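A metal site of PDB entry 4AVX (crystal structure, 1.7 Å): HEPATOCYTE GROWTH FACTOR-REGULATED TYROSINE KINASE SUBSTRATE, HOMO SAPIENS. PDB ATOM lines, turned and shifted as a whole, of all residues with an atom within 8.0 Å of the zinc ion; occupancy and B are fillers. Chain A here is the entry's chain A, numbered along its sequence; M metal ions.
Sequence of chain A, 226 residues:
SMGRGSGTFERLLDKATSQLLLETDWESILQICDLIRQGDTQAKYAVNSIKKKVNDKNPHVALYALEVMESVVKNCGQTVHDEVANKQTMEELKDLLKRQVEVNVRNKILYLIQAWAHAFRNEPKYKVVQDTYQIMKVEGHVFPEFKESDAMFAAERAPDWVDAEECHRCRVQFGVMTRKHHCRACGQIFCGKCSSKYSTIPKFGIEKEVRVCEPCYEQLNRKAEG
The side-chain sulfur of Cys 194 sits close to the guanidinium group of Arg 169 (3.7 Å). SG of Cys 170 lies close to N of Val 172 (3.6 Å). N of Cys 167 sits at hydrogen-bond distance from O of Val 172, at 2.9 Å. SG of Cys 167 lies close to N of Arg 169. The side-chain sulfur (SG) of Cys 191 sits close to the backbone NH (N) of Lys 193, at 3.6 Å. The backbone carbonyl oxygen (O) of Cys 191 sits at hydrogen-bond distance from the side-chain hydroxyl (OG) of Ser 195, at 2.9 Å.
The zinc ion is bound by SG of Cys 194 (2.3 Å), SG of Cys 170 (2.3 Å), SG of Cys 167 (2.4 Å) and SG of Cys 191 (2.4 Å). The zinc ion has four donor atoms within binding distance.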
ATOM      1  N   GLU A 166       6.981   2.676   0.930  1.00  0.00           N
ATOM      2  CA  GLU A 166       8.001   3.718   0.925  1.00  0.00           C
ATOM      3  C   GLU A 166       8.301   4.264  -0.503  1.00  0.00           C
ATOM      4  O   GLU A 166       8.010   3.575  -1.516  1.00  0.00           O
ATOM      5  CB  GLU A 166       9.318   3.219   1.520  1.00  0.00           C
ATOM      6  CG  GLU A 166       9.926   2.073   0.741  1.00  0.00           C
ATOM      7  CD  GLU A 166      11.152   1.507   1.432  1.00  0.00           C
ATOM      8  OE1 GLU A 166      11.352   1.798   2.635  1.00  0.00           O
ATOM      9  OE2 GLU A 166      11.915   0.781   0.752  1.00  0.00           O
ATOM     10  N   CYS A 167       8.822   5.487  -0.560  1.00  0.00           N
ATOM     11  CA  CYS A 167       9.147   6.124  -1.838  1.00  0.00           C
ATOM     12  C   CYS A 167      10.268   5.348  -2.552  1.00  0.00           C
ATOM     13  O   CYS A 167      11.286   4.973  -1.951  1.00  0.00           O
ATOM     14  CB  CYS A 167       9.568   7.539  -1.597  1.00  0.00           C
ATOM     15  SG  CYS A 167      10.127   8.397  -3.075  1.00  0.00           S
ATOM     16  N   HIS A 168      10.090   5.140  -3.853  1.00  0.00           N
ATOM     17  CA  HIS A 168      11.031   4.365  -4.615  1.00  0.00           C
ATOM     18  C   HIS A 168      12.373   5.026  -4.668  1.00  0.00           C
ATOM     19  O   HIS A 168      13.395   4.321  -4.664  1.00  0.00           O
ATOM     20  CB  HIS A 168      10.458   4.137  -6.010  1.00  0.00           C
ATOM     21  CG  HIS A 168      11.382   3.408  -6.916  1.00  0.00           C
ATOM     22  ND1 HIS A 168      11.603   2.075  -6.778  1.00  0.00           N
ATOM     23  CD2 HIS A 168      12.162   3.854  -7.987  1.00  0.00           C
ATOM     24  CE1 HIS A 168      12.477   1.684  -7.748  1.00  0.00           C
ATOM     25  NE2 HIS A 168      12.824   2.779  -8.471  1.00  0.00           N
ATOM     26  N   ARG A 169      12.411   6.354  -4.616  1.00  0.00           N
ATOM     27  CA  ARG A 169      13.670   7.097  -4.682  1.00  0.00           C
ATOM     28  C   ARG A 169      14.321   7.283  -3.320  1.00  0.00           C
ATOM     29  O   ARG A 169      15.427   6.782  -3.077  1.00  0.00           O
ATOM     30  CB  ARG A 169      13.475   8.438  -5.404  1.00  0.00           C
ATOM     31  CG  ARG A 169      14.653   9.411  -5.246  1.00  0.00           C
ATOM     32  CD  ARG A 169      14.673  10.469  -6.321  1.00  0.00           C
ATOM     33  NE  ARG A 169      15.199  11.725  -5.790  1.00  0.00           N
ATOM     34  CZ  ARG A 169      15.096  12.917  -6.391  1.00  0.00           C
ATOM     35  NH1 ARG A 169      14.497  13.042  -7.574  1.00  0.00           N
ATOM     36  NH2 ARG A 169      15.604  13.995  -5.799  1.00  0.00           N
ATOM     37  N   CYS A 170      13.642   7.966  -2.403  1.00  0.00           N
ATOM     38  CA  CYS A 170      14.232   8.348  -1.122  1.00  0.00           C
ATOM     39  C   CYS A 170      13.840   7.446   0.045  1.00  0.00           C
ATOM     40  O   CYS A 170      14.414   7.571   1.152  1.00  0.00           O
ATOM     41  CB  CYS A 170      13.877   9.804  -0.794  1.00  0.00           C
ATOM     42  SG  CYS A 170      12.152  10.072  -0.305  1.00  0.00           S
ATOM     43  N   ARG A 171      12.908   6.534  -0.195  1.00  0.00           N
ATOM     44  CA  ARG A 171      12.517   5.499   0.783  1.00  0.00           C
ATOM     45  C   ARG A 171      11.835   6.070   2.017  1.00  0.00           C
ATOM     46  O   ARG A 171      11.610   5.333   2.962  1.00  0.00           O
ATOM     47  CB  ARG A 171      13.725   4.615   1.178  1.00  0.00           C
ATOM     48  CG  ARG A 171      14.404   3.929  -0.001  1.00  0.00           C
ATOM     49  CD  ARG A 171      13.567   2.796  -0.555  1.00  0.00           C
ATOM     50  NE  ARG A 171      13.977   2.398  -1.906  1.00  0.00           N
ATOM     51  CZ  ARG A 171      13.292   1.582  -2.707  1.00  0.00           C
ATOM     52  NH1 ARG A 171      12.134   1.059  -2.323  1.00  0.00           N
ATOM     53  NH2 ARG A 171      13.777   1.283  -3.923  1.00  0.00           N
ATOM     54  N   VAL A 172      11.469   7.344   1.997  1.00  0.00           N
ATOM     55  CA  VAL A 172      10.593   7.883   3.041  1.00  0.00           C
ATOM     56  C   VAL A 172       9.336   7.000   3.118  1.00  0.00           C
ATOM     57  O   VAL A 172       8.803   6.563   2.111  1.00  0.00           O
ATOM     58  CB  VAL A 172      10.255   9.374   2.845  1.00  0.00           C
ATOM     59  CG1 VAL A 172       9.188   9.582   1.756  1.00  0.00           C
ATOM     60  CG2 VAL A 172       9.807  10.013   4.161  1.00  0.00           C
ATOM     61  N   GLN A 173       8.891   6.717   4.354  1.00  0.00           N
ATOM     62  CA  GLN A 173       7.750   5.845   4.591  1.00  0.00           C
ATOM     63  C   GLN A 173       6.481   6.680   4.374  1.00  0.00           C
ATOM     64  O   GLN A 173       6.353   7.798   4.886  1.00  0.00           O
ATOM     65  CB  GLN A 173       7.766   5.221   5.992  1.00  0.00           C
ATOM     66  CG  GLN A 173       9.053   4.456   6.347  1.00  0.00           C
ATOM     67  CD  GLN A 173       9.335   3.244   5.447  1.00  0.00           C
ATOM     68  OE1 GLN A 173       8.499   2.360   5.313  1.00  0.00           O
ATOM     69  NE2 GLN A 173      10.542   3.196   4.879  1.00  0.00           N
ATOM     70  N   PHE A 174       5.588   6.126   3.584  1.00  0.00           N
ATOM     71  CA  PHE A 174       4.297   6.724   3.355  1.00  0.00           C
ATOM     72  C   PHE A 174       3.462   6.636   4.632  1.00  0.00           C
ATOM     73  O   PHE A 174       3.630   5.717   5.429  1.00  0.00           O
ATOM     74  CB  PHE A 174       3.541   6.068   2.209  1.00  0.00           C
ATOM     75  CG  PHE A 174       4.214   6.280   0.845  1.00  0.00           C
ATOM     76  CD1 PHE A 174       4.449   7.596   0.398  1.00  0.00           C
ATOM     77  CD2 PHE A 174       4.656   5.231   0.070  1.00  0.00           C
ATOM     78  CE1 PHE A 174       5.070   7.817  -0.862  1.00  0.00           C
ATOM     79  CE2 PHE A 174       5.284   5.441  -1.161  1.00  0.00           C
ATOM     80  CZ  PHE A 174       5.499   6.727  -1.604  1.00  0.00           C
ATOM     81  N   THR A 178       2.294  11.654   4.569  1.00  0.00           N
ATOM     82  CA  THR A 178       3.330  11.508   3.531  1.00  0.00           C
ATOM     83  C   THR A 178       2.687  10.687   2.479  1.00  0.00           C
ATOM     84  O   THR A 178       2.751   9.446   2.531  1.00  0.00           O
ATOM     85  CB  THR A 178       4.639  10.858   4.080  1.00  0.00           C
ATOM     86  OG1 THR A 178       5.165  11.668   5.128  1.00  0.00           O
ATOM     87  CG2 THR A 178       5.730  10.687   2.979  1.00  0.00           C
ATOM     88  N   ILE A 189       6.273   4.278  -7.465  1.00  0.00           N
ATOM     89  CA  ILE A 189       5.576   5.047  -6.444  1.00  0.00           C
ATOM     90  C   ILE A 189       6.550   5.952  -5.708  1.00  0.00           C
ATOM     91  O   ILE A 189       7.711   5.566  -5.433  1.00  0.00           O
ATOM     92  CB  ILE A 189       4.813   4.084  -5.467  1.00  0.00           C
ATOM     93  CG1 ILE A 189       3.762   4.845  -4.644  1.00  0.00           C
ATOM     94  CG2 ILE A 189       5.793   3.310  -4.588  1.00  0.00           C
ATOM     95  CD1 ILE A 189       2.831   3.908  -3.869  1.00  0.00           C
ATOM     96  N   PHE A 190       6.139   7.193  -5.521  1.00  0.00           N
ATOM     97  CA  PHE A 190       6.995   8.233  -5.026  1.00  0.00           C
ATOM     98  C   PHE A 190       6.310   9.143  -4.036  1.00  0.00           C
ATOM     99  O   PHE A 190       5.091   9.363  -4.118  1.00  0.00           O
ATOM    100  CB  PHE A 190       7.524   9.121  -6.170  1.00  0.00           C
ATOM    101  CG  PHE A 190       8.349   8.396  -7.183  1.00  0.00           C
ATOM    102  CD1 PHE A 190       7.760   7.790  -8.307  1.00  0.00           C
ATOM    103  CD2 PHE A 190       9.726   8.285  -7.036  1.00  0.00           C
ATOM    104  CE1 PHE A 190       8.540   7.109  -9.213  1.00  0.00           C
ATOM    105  CE2 PHE A 190      10.484   7.567  -7.925  1.00  0.00           C
ATOM    106  CZ  PHE A 190       9.890   7.010  -9.034  1.00  0.00           C
ATOM    107  N   CYS A 191       7.087   9.757  -3.174  1.00  0.00           N
ATOM    108  CA  CYS A 191       6.652  10.927  -2.492  1.00  0.00           C
ATOM    109  C   CYS A 191       6.542  12.136  -3.428  1.00  0.00           C
ATOM    110  O   CYS A 191       7.050  12.144  -4.556  1.00  0.00           O
ATOM    111  CB  CYS A 191       7.538  11.201  -1.257  1.00  0.00           C
ATOM    112  SG  CYS A 191       9.059  12.012  -1.699  1.00  0.00           S
ATOM    113  N   GLY A 192       5.847  13.163  -2.961  1.00  0.00           N
ATOM    114  CA  GLY A 192       5.656  14.377  -3.753  1.00  0.00           C
ATOM    115  C   GLY A 192       6.948  15.058  -4.151  1.00  0.00           C
ATOM    116  O   GLY A 192       7.101  15.431  -5.323  1.00  0.00           O
ATOM    117  N   LYS A 193       7.925  15.097  -3.255  1.00  0.00           N
ATOM    118  CA  LYS A 193       9.226  15.751  -3.583  1.00  0.00           C
ATOM    119  C   LYS A 193      10.000  15.048  -4.680  1.00  0.00           C
ATOM    120  O   LYS A 193      10.805  15.662  -5.391  1.00  0.00           O
ATOM    121  CB  LYS A 193      10.085  15.968  -2.312  1.00  0.00           C
ATOM    122  CG  LYS A 193       9.518  17.027  -1.354  1.00  0.00           C
ATOM    123  CD  LYS A 193      10.267  17.115  -0.015  1.00  0.00           C
ATOM    124  N   CYS A 194       9.802  13.736  -4.800  1.00  0.00           N
ATOM    125  CA  CYS A 194      10.505  12.918  -5.730  1.00  0.00           C
ATOM    126  C   CYS A 194       9.748  12.779  -7.089  1.00  0.00           C
ATOM    127  O   CYS A 194      10.272  12.226  -8.048  1.00  0.00           O
ATOM    128  CB  CYS A 194      10.772  11.530  -5.086  1.00  0.00           C
ATOM    129  SG  CYS A 194      12.092  11.521  -3.787  1.00  0.00           S
ATOM    130  N   SER A 195       8.533  13.314  -7.141  1.00  0.00           N
ATOM    131  CA  SER A 195       7.675  13.220  -8.358  1.00  0.00           C
ATOM    132  C   SER A 195       6.973  14.547  -8.654  1.00  0.00           C
ATOM    133  O   SER A 195       5.780  14.592  -8.890  1.00  0.00           O
ATOM    134  CB  SER A 195       6.672  12.086  -8.232  1.00  0.00           C
ATOM    135  OG  SER A 195       5.813  12.255  -7.125  1.00  0.00           O
HETATM  136 ZN    ZN M   1      10.876  10.491  -2.167  1.00  0.00          ZN
